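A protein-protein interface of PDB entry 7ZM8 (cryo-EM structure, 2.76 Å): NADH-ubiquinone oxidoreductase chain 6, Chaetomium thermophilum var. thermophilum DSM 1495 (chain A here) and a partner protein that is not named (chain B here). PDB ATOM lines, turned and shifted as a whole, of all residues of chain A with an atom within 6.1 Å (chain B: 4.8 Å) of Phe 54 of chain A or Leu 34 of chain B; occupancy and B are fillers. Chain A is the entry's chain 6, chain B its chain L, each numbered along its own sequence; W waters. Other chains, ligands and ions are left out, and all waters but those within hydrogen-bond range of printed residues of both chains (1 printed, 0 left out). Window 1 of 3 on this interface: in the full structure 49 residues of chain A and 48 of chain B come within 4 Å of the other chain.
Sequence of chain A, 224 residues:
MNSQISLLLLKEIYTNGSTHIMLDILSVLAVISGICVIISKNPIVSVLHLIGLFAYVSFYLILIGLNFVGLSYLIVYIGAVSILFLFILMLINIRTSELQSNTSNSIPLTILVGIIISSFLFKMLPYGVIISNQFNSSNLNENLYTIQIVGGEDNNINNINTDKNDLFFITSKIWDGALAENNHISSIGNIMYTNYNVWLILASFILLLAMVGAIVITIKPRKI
Printed residues of chain A that touch a printed residue of chain B: Leu 50, Phe 54, Val 57, Tyr 73 and Tyr 77. Hydrophobic or aromatic side chains of chain A within 4 Å of the printed part of chain B: Leu 50, Phe 54, Val 57, Tyr 73 and Tyr 77. Hydrophobic or aromatic side chains of chain B that line the printed part of chain A: Ile 31, Leu 34 and Phe 38. Among the printed residues, 7 pairs touch across the chains.
His 49 of chain A touches none of the printed residues of chain B. Printed residues of chain B within 4 Å of Leu 50 of chain A: Ile 31 (3.6 Å). Gly 52 of chain A touches none of the printed residues of chain B. Phe 54 of chain A touches one residue of chain B. Of the printed residues of chain A, Glu 30 of chain B touches Tyr 77 (3.5 Å). The nearest residue of chain B that does not touch Phe 54 of chain A is Glu 30 of chain B (4.3 Å).
Water W1 lies within hydrogen-bond range of the backbone carbonyl oxygen of Glu 30 of chain B (3.0 Å) and the side-chain hydroxyl of Tyr 77 of chain A (3.3 Å).
The backbone carbonyl oxygen of Ile 31 of chain B lies within hydrogen-bond range of the side-chain hydroxyl of Ser 35 of chain B (2.6 Å). O of Phe 54 of chain A lies within hydrogen-bond range of OG of Ser 58 of chain A, 2.7 Å away.
Among the printed residues, pairs that only touch across the chains: Tyr 77 of chain A with Glu 30 of chain B, Leu 50 of chain A with Ile 31 of chain B, Phe 54 of chain A with Leu 34 of chain B, Val 57 of chain A with Leu 34 of chain B, Tyr 73 of chain A with Leu 34 of chain B and Val 57 of chain A with Phe 38 of chain B.
OG1 of Thr 37 of chain B sits at hydrogen-bond distance from OH of Tyr 73 of chain A, at 2.7 Å.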
ATOM      1  N   SER A  33      -3.842  -6.866  28.953  1.00  0.00           N
ATOM      2  CA  SER A  33      -4.835  -6.139  28.167  1.00  0.00           C
ATOM      3  C   SER A  33      -6.198  -6.147  28.850  1.00  0.00           C
ATOM      4  O   SER A  33      -7.036  -5.283  28.577  1.00  0.00           O
ATOM      5  CB  SER A  33      -4.934  -6.726  26.759  1.00  0.00           C
ATOM      6  OG  SER A  33      -5.797  -7.841  26.728  1.00  0.00           O
ATOM      7  N   HIS A  49      -8.566  -2.610  23.153  1.00  0.00           N
ATOM      8  CA  HIS A  49      -7.897  -3.545  24.099  1.00  0.00           C
ATOM      9  C   HIS A  49      -8.728  -4.825  24.204  1.00  0.00           C
ATOM     10  O   HIS A  49      -8.146  -5.862  24.539  1.00  0.00           O
ATOM     11  CB  HIS A  49      -7.665  -2.879  25.461  1.00  0.00           C
ATOM     12  CG  HIS A  49      -6.584  -1.855  25.465  1.00  0.00           C
ATOM     13  ND1 HIS A  49      -5.299  -2.137  25.052  1.00  0.00           N
ATOM     14  CD2 HIS A  49      -6.582  -0.564  25.851  1.00  0.00           C
ATOM     15  CE1 HIS A  49      -4.558  -1.057  25.165  1.00  0.00           C
ATOM     16  NE2 HIS A  49      -5.318  -0.080  25.652  1.00  0.00           N
ATOM     17  N   LEU A  50     -10.040  -4.748  23.947  1.00  0.00           N
ATOM     18  CA  LEU A  50     -10.840  -5.961  23.905  1.00  0.00           C
ATOM     19  C   LEU A  50     -10.549  -6.762  22.644  1.00  0.00           C
ATOM     20  O   LEU A  50     -10.516  -7.996  22.680  1.00  0.00           O
ATOM     21  CB  LEU A  50     -12.320  -5.612  23.997  1.00  0.00           C
ATOM     22  CG  LEU A  50     -13.235  -6.797  24.283  1.00  0.00           C
ATOM     23  CD1 LEU A  50     -13.082  -7.235  25.720  1.00  0.00           C
ATOM     24  CD2 LEU A  50     -14.670  -6.443  23.984  1.00  0.00           C
ATOM     25  N   ILE A  51     -10.348  -6.079  21.517  1.00  0.00           N
ATOM     26  CA  ILE A  51      -9.932  -6.768  20.301  1.00  0.00           C
ATOM     27  C   ILE A  51      -8.589  -7.446  20.520  1.00  0.00           C
ATOM     28  O   ILE A  51      -8.346  -8.551  20.023  1.00  0.00           O
ATOM     29  CB  ILE A  51      -9.890  -5.788  19.112  1.00  0.00           C
ATOM     30  CG1 ILE A  51     -11.251  -5.136  18.910  1.00  0.00           C
ATOM     31  CG2 ILE A  51      -9.500  -6.504  17.837  1.00  0.00           C
ATOM     32  CD1 ILE A  51     -11.205  -3.887  18.082  1.00  0.00           C
ATOM     33  N   GLY A  52      -7.698  -6.800  21.269  1.00  0.00           N
ATOM     34  CA  GLY A  52      -6.431  -7.429  21.595  1.00  0.00           C
ATOM     35  C   GLY A  52      -6.599  -8.669  22.451  1.00  0.00           C
ATOM     36  O   GLY A  52      -5.988  -9.704  22.182  1.00  0.00           O
ATOM     37  N   LEU A  53      -7.444  -8.612  23.471  1.00  0.00           N
ATOM     38  CA  LEU A  53      -7.692  -9.764  24.370  1.00  0.00           C
ATOM     39  C   LEU A  53      -8.282 -10.948  23.601  1.00  0.00           C
ATOM     40  O   LEU A  53      -7.809 -12.065  23.809  1.00  0.00           O
ATOM     41  CB  LEU A  53      -8.647  -9.285  25.470  1.00  0.00           C
ATOM     42  CG  LEU A  53      -9.286 -10.369  26.337  1.00  0.00           C
ATOM     43  CD1 LEU A  53      -8.237 -11.131  27.131  1.00  0.00           C
ATOM     44  CD2 LEU A  53     -10.321  -9.771  27.273  1.00  0.00           C
ATOM     45  N   PHE A  54      -9.257 -10.712  22.734  1.00  0.00           N
ATOM     46  CA  PHE A  54      -9.947 -11.805  22.007  1.00  0.00           C
ATOM     47  C   PHE A  54      -8.941 -12.560  21.149  1.00  0.00           C
ATOM     48  O   PHE A  54      -9.116 -13.765  20.992  1.00  0.00           O
ATOM     49  CB  PHE A  54     -11.151 -11.263  21.230  1.00  0.00           C
ATOM     50  CG  PHE A  54     -12.433 -11.223  22.019  1.00  0.00           C
ATOM     51  CD1 PHE A  54     -13.033 -12.392  22.451  1.00  0.00           C
ATOM     52  CD2 PHE A  54     -13.045 -10.020  22.323  1.00  0.00           C
ATOM     53  CE1 PHE A  54     -14.216 -12.358  23.172  1.00  0.00           C
ATOM     54  CE2 PHE A  54     -14.226  -9.987  23.047  1.00  0.00           C
ATOM     55  CZ  PHE A  54     -14.807 -11.155  23.476  1.00  0.00           C
ATOM     56  N   ALA A  55      -7.904 -11.880  20.659  1.00  0.00           N
ATOM     57  CA  ALA A  55      -6.900 -12.514  19.789  1.00  0.00           C
ATOM     58  C   ALA A  55      -5.900 -13.303  20.630  1.00  0.00           C
ATOM     59  O   ALA A  55      -5.560 -14.396  20.208  1.00  0.00           O
ATOM     60  CB  ALA A  55      -6.204 -11.445  19.010  1.00  0.00           C
ATOM     61  N   TYR A  56      -5.519 -12.826  21.805  1.00  0.00           N
ATOM     62  CA  TYR A  56      -4.620 -13.621  22.681  1.00  0.00           C
ATOM     63  C   TYR A  56      -5.251 -14.976  23.021  1.00  0.00           C
ATOM     64  O   TYR A  56      -4.530 -15.974  22.941  1.00  0.00           O
ATOM     65  CB  TYR A  56      -4.260 -12.821  23.931  1.00  0.00           C
ATOM     66  CG  TYR A  56      -3.521 -11.534  23.673  1.00  0.00           C
ATOM     67  CD1 TYR A  56      -2.523 -11.463  22.718  1.00  0.00           C
ATOM     68  CD2 TYR A  56      -3.811 -10.389  24.394  1.00  0.00           C
ATOM     69  CE1 TYR A  56      -1.838 -10.284  22.476  1.00  0.00           C
ATOM     70  CE2 TYR A  56      -3.134  -9.205  24.167  1.00  0.00           C
ATOM     71  CZ  TYR A  56      -2.144  -9.152  23.206  1.00  0.00           C
ATOM     72  OH  TYR A  56      -1.475  -7.984  22.980  1.00  0.00           O
ATOM     73  N   VAL A  57      -6.524 -14.997  23.407  1.00  0.00           N
ATOM     74  CA  VAL A  57      -7.267 -16.242  23.751  1.00  0.00           C
ATOM     75  C   VAL A  57      -7.411 -17.118  22.506  1.00  0.00           C
ATOM     76  O   VAL A  57      -7.271 -18.337  22.620  1.00  0.00           O
ATOM     77  CB  VAL A  57      -8.630 -15.870  24.364  1.00  0.00           C
ATOM     78  CG1 VAL A  57      -9.491 -17.091  24.652  1.00  0.00           C
ATOM     79  CG2 VAL A  57      -8.462 -15.023  25.615  1.00  0.00           C
ATOM     80  N   SER A  58      -7.671 -16.500  21.356  1.00  0.00           N
ATOM     81  CA  SER A  58      -7.842 -17.258  20.099  1.00  0.00           C
ATOM     82  C   SER A  58      -6.545 -17.982  19.779  1.00  0.00           C
ATOM     83  O   SER A  58      -6.606 -19.162  19.438  1.00  0.00           O
ATOM     84  CB  SER A  58      -8.204 -16.320  19.002  1.00  0.00           C
ATOM     85  OG  SER A  58      -9.479 -15.744  19.230  1.00  0.00           O
ATOM     86  N   PHE A  59      -5.420 -17.296  19.929  1.00  0.00           N
ATOM     87  CA  PHE A  59      -4.091 -17.887  19.653  1.00  0.00           C
ATOM     88  C   PHE A  59      -3.794 -18.999  20.653  1.00  0.00           C
ATOM     89  O   PHE A  59      -3.256 -20.019  20.231  1.00  0.00           O
ATOM     90  CB  PHE A  59      -3.020 -16.800  19.670  1.00  0.00           C
ATOM     91  CG  PHE A  59      -3.211 -15.693  18.666  1.00  0.00           C
ATOM     92  CD1 PHE A  59      -3.955 -15.896  17.515  1.00  0.00           C
ATOM     93  CD2 PHE A  59      -2.638 -14.450  18.868  1.00  0.00           C
ATOM     94  CE1 PHE A  59      -4.134 -14.875  16.596  1.00  0.00           C
ATOM     95  CE2 PHE A  59      -2.812 -13.432  17.944  1.00  0.00           C
ATOM     96  CZ  PHE A  59      -3.559 -13.646  16.812  1.00  0.00           C
ATOM     97  N   TYR A  73     -13.687 -17.841  16.763  1.00  0.00           N
ATOM     98  CA  TYR A  73     -13.634 -16.700  17.698  1.00  0.00           C
ATOM     99  C   TYR A  73     -13.074 -15.502  16.955  1.00  0.00           C
ATOM    100  O   TYR A  73     -13.620 -14.415  17.099  1.00  0.00           O
ATOM    101  CB  TYR A  73     -12.638 -16.988  18.816  1.00  0.00           C
ATOM    102  CG  TYR A  73     -13.166 -17.676  20.043  1.00  0.00           C
ATOM    103  CD1 TYR A  73     -13.987 -17.024  20.945  1.00  0.00           C
ATOM    104  CD2 TYR A  73     -12.782 -18.969  20.329  1.00  0.00           C
ATOM    105  CE1 TYR A  73     -14.451 -17.661  22.081  1.00  0.00           C
ATOM    106  CE2 TYR A  73     -13.243 -19.627  21.450  1.00  0.00           C
ATOM    107  CZ  TYR A  73     -14.073 -18.968  22.332  1.00  0.00           C
ATOM    108  OH  TYR A  73     -14.498 -19.641  23.434  1.00  0.00           O
ATOM    109  N   LEU A  74     -12.011 -15.710  16.185  1.00  0.00           N
ATOM    110  CA  LEU A  74     -11.378 -14.599  15.434  1.00  0.00           C
ATOM    111  C   LEU A  74     -12.355 -14.044  14.392  1.00  0.00           C
ATOM    112  O   LEU A  74     -12.507 -12.821  14.350  1.00  0.00           O
ATOM    113  CB  LEU A  74     -10.092 -15.114  14.776  1.00  0.00           C
ATOM    114  CG  LEU A  74      -8.846 -15.150  15.650  1.00  0.00           C
ATOM    115  CD1 LEU A  74      -7.678 -15.727  14.871  1.00  0.00           C
ATOM    116  CD2 LEU A  74      -8.506 -13.762  16.156  1.00  0.00           C
ATOM    117  N   TYR A  77     -15.747 -12.629  16.877  1.00  0.00           N
ATOM    118  CA  TYR A  77     -15.498 -11.525  17.840  1.00  0.00           C
ATOM    119  C   TYR A  77     -14.762 -10.354  17.207  1.00  0.00           C
ATOM    120  O   TYR A  77     -15.231  -9.227  17.341  1.00  0.00           O
ATOM    121  CB  TYR A  77     -14.877 -12.041  19.137  1.00  0.00           C
ATOM    122  CG  TYR A  77     -15.888 -12.778  19.971  1.00  0.00           C
ATOM    123  CD1 TYR A  77     -16.939 -12.102  20.564  1.00  0.00           C
ATOM    124  CD2 TYR A  77     -15.832 -14.150  20.115  1.00  0.00           C
ATOM    125  CE1 TYR A  77     -17.894 -12.769  21.308  1.00  0.00           C
ATOM    126  CE2 TYR A  77     -16.775 -14.832  20.862  1.00  0.00           C
ATOM    127  CZ  TYR A  77     -17.811 -14.139  21.459  1.00  0.00           C
ATOM    128  OH  TYR A  77     -18.740 -14.810  22.194  1.00  0.00           O
ATOM    129  N   ILE A  78     -13.671 -10.624  16.506  1.00  0.00           N
ATOM    130  CA  ILE A  78     -12.887  -9.491  15.957  1.00  0.00           C
ATOM    131  C   ILE A  78     -13.511  -9.102  14.623  1.00  0.00           C
ATOM    132  O   ILE A  78     -13.695  -7.917  14.377  1.00  0.00           O
ATOM    133  CB  ILE A  78     -11.396  -9.861  15.875  1.00  0.00           C
ATOM    134  CG1 ILE A  78     -10.814 -10.122  17.265  1.00  0.00           C
ATOM    135  CG2 ILE A  78     -10.594  -8.820  15.116  1.00  0.00           C
ATOM    136  CD1 ILE A  78      -9.339 -10.401  17.260  1.00  0.00           C
ATOM    137  N   GLU B  30     -19.115  -9.289  28.089  1.00  0.00           N
ATOM    138  CA  GLU B  30     -18.421 -10.095  27.062  1.00  0.00           C
ATOM    139  C   GLU B  30     -17.135 -10.741  27.591  1.00  0.00           C
ATOM    140  O   GLU B  30     -16.870 -11.883  27.220  1.00  0.00           O
ATOM    141  CB  GLU B  30     -18.210  -9.213  25.837  1.00  0.00           C
ATOM    142  CG  GLU B  30     -19.443  -9.124  24.964  1.00  0.00           C
ATOM    143  CD  GLU B  30     -19.133  -9.023  23.483  1.00  0.00           C
ATOM    144  OE1 GLU B  30     -18.627  -7.966  23.060  1.00  0.00           O
ATOM    145  OE2 GLU B  30     -19.385 -10.008  22.759  1.00  0.00           O
ATOM    146  N   ILE B  31     -16.366 -10.033  28.417  1.00  0.00           N
ATOM    147  CA  ILE B  31     -15.146 -10.618  29.043  1.00  0.00           C
ATOM    148  C   ILE B  31     -15.571 -11.803  29.905  1.00  0.00           C
ATOM    149  O   ILE B  31     -14.882 -12.822  29.848  1.00  0.00           O
ATOM    150  CB  ILE B  31     -14.379  -9.563  29.868  1.00  0.00           C
ATOM    151  CG1 ILE B  31     -13.979  -8.355  29.022  1.00  0.00           C
ATOM    152  CG2 ILE B  31     -13.172 -10.172  30.561  1.00  0.00           C
ATOM    153  CD1 ILE B  31     -13.281  -7.270  29.799  1.00  0.00           C
ATOM    154  N   MET B  32     -16.674 -11.675  30.647  1.00  0.00           N
ATOM    155  CA  MET B  32     -17.182 -12.795  31.479  1.00  0.00           C
ATOM    156  C   MET B  32     -17.621 -13.980  30.607  1.00  0.00           C
ATOM    157  O   MET B  32     -17.311 -15.108  30.978  1.00  0.00           O
ATOM    158  CB  MET B  32     -18.302 -12.347  32.421  1.00  0.00           C
ATOM    159  CG  MET B  32     -17.828 -11.578  33.627  1.00  0.00           C
ATOM    160  SD  MET B  32     -19.236 -11.103  34.656  1.00  0.00           S
ATOM    161  CE  MET B  32     -19.887  -9.721  33.724  1.00  0.00           C
ATOM    162  N   LEU B  33     -18.286 -13.734  29.488  1.00  0.00           N
ATOM    163  CA  LEU B  33     -18.680 -14.818  28.552  1.00  0.00           C
ATOM    164  C   LEU B  33     -17.438 -15.509  27.989  1.00  0.00           C
ATOM    165  O   LEU B  33     -17.468 -16.735  27.916  1.00  0.00           O
ATOM    166  CB  LEU B  33     -19.568 -14.226  27.457  1.00  0.00           C
ATOM    167  CG  LEU B  33     -20.880 -13.616  27.945  1.00  0.00           C
ATOM    168  CD1 LEU B  33     -21.593 -12.876  26.826  1.00  0.00           C
ATOM    169  CD2 LEU B  33     -21.782 -14.671  28.556  1.00  0.00           C
ATOM    170  N   LEU B  34     -16.394 -14.757  27.630  1.00  0.00           N
ATOM    171  CA  LEU B  34     -15.140 -15.327  27.085  1.00  0.00           C
ATOM    172  C   LEU B  34     -14.479 -16.230  28.123  1.00  0.00           C
ATOM    173  O   LEU B  34     -13.980 -17.288  27.752  1.00  0.00           O
ATOM    174  CB  LEU B  34     -14.206 -14.192  26.661  1.00  0.00           C
ATOM    175  CG  LEU B  34     -12.841 -14.612  26.126  1.00  0.00           C
ATOM    176  CD1 LEU B  34     -12.983 -15.352  24.807  1.00  0.00           C
ATOM    177  CD2 LEU B  34     -11.940 -13.402  25.962  1.00  0.00           C
ATOM    178  N   SER B  35     -14.449 -15.804  29.375  1.00  0.00           N
ATOM    179  CA  SER B  35     -13.784 -16.602  30.432  1.00  0.00           C
ATOM    180  C   SER B  35     -14.515 -17.933  30.590  1.00  0.00           C
ATOM    181  O   SER B  35     -13.842 -18.963  30.682  1.00  0.00           O
ATOM    182  CB  SER B  35     -13.781 -15.833  31.725  1.00  0.00           C
ATOM    183  OG  SER B  35     -13.625 -14.447  31.486  1.00  0.00           O
ATOM    184  N   ILE B  36     -15.846 -17.896  30.640  1.00  0.00           N
ATOM    185  CA  ILE B  36     -16.678 -19.115  30.840  1.00  0.00           C
ATOM    186  C   ILE B  36     -16.550 -20.033  29.623  1.00  0.00           C
ATOM    187  O   ILE B  36     -16.379 -21.237  29.828  1.00  0.00           O
ATOM    188  CB  ILE B  36     -18.135 -18.720  31.199  1.00  0.00           C
ATOM    189  CG1 ILE B  36     -18.234 -18.051  32.571  1.00  0.00           C
ATOM    190  CG2 ILE B  36     -19.092 -19.891  31.074  1.00  0.00           C
ATOM    191  CD1 ILE B  36     -19.485 -17.229  32.745  1.00  0.00           C
ATOM    192  N   THR B  37     -16.581 -19.485  28.409  1.00  0.00           N
ATOM    193  CA  THR B  37     -16.382 -20.333  27.205  1.00  0.00           C
ATOM    194  C   THR B  37     -14.972 -20.934  27.194  1.00  0.00           C
ATOM    195  O   THR B  37     -14.864 -22.120  26.866  1.00  0.00           O
ATOM    196  CB  THR B  37     -16.802 -19.617  25.913  1.00  0.00           C
ATOM    197  OG1 THR B  37     -16.603 -20.509  24.817  1.00  0.00           O
ATOM    198  CG2 THR B  37     -16.046 -18.335  25.653  1.00  0.00           C
ATOM    199  N   PHE B  38     -13.952 -20.157  27.550  1.00  0.00           N
ATOM    200  CA  PHE B  38     -12.545 -20.620  27.580  1.00  0.00           C
ATOM    201  C   PHE B  38     -12.399 -21.731  28.623  1.00  0.00           C
ATOM    202  O   PHE B  38     -11.654 -22.684  28.359  1.00  0.00           O
ATOM    203  CB  PHE B  38     -11.662 -19.398  27.822  1.00  0.00           C
ATOM    204  CG  PHE B  38     -10.174 -19.566  27.653  1.00  0.00           C
ATOM    205  CD1 PHE B  38      -9.649 -20.422  26.702  1.00  0.00           C
ATOM    206  CD2 PHE B  38      -9.300 -18.818  28.421  1.00  0.00           C
ATOM    207  CE1 PHE B  38      -8.279 -20.551  26.547  1.00  0.00           C
ATOM    208  CE2 PHE B  38      -7.930 -18.946  28.265  1.00  0.00           C
ATOM    209  CZ  PHE B  38      -7.424 -19.813  27.329  1.00  0.00           C
HETATM  210  O   HOH W   1     -18.049 -12.585  24.584  1.00  0.00           O
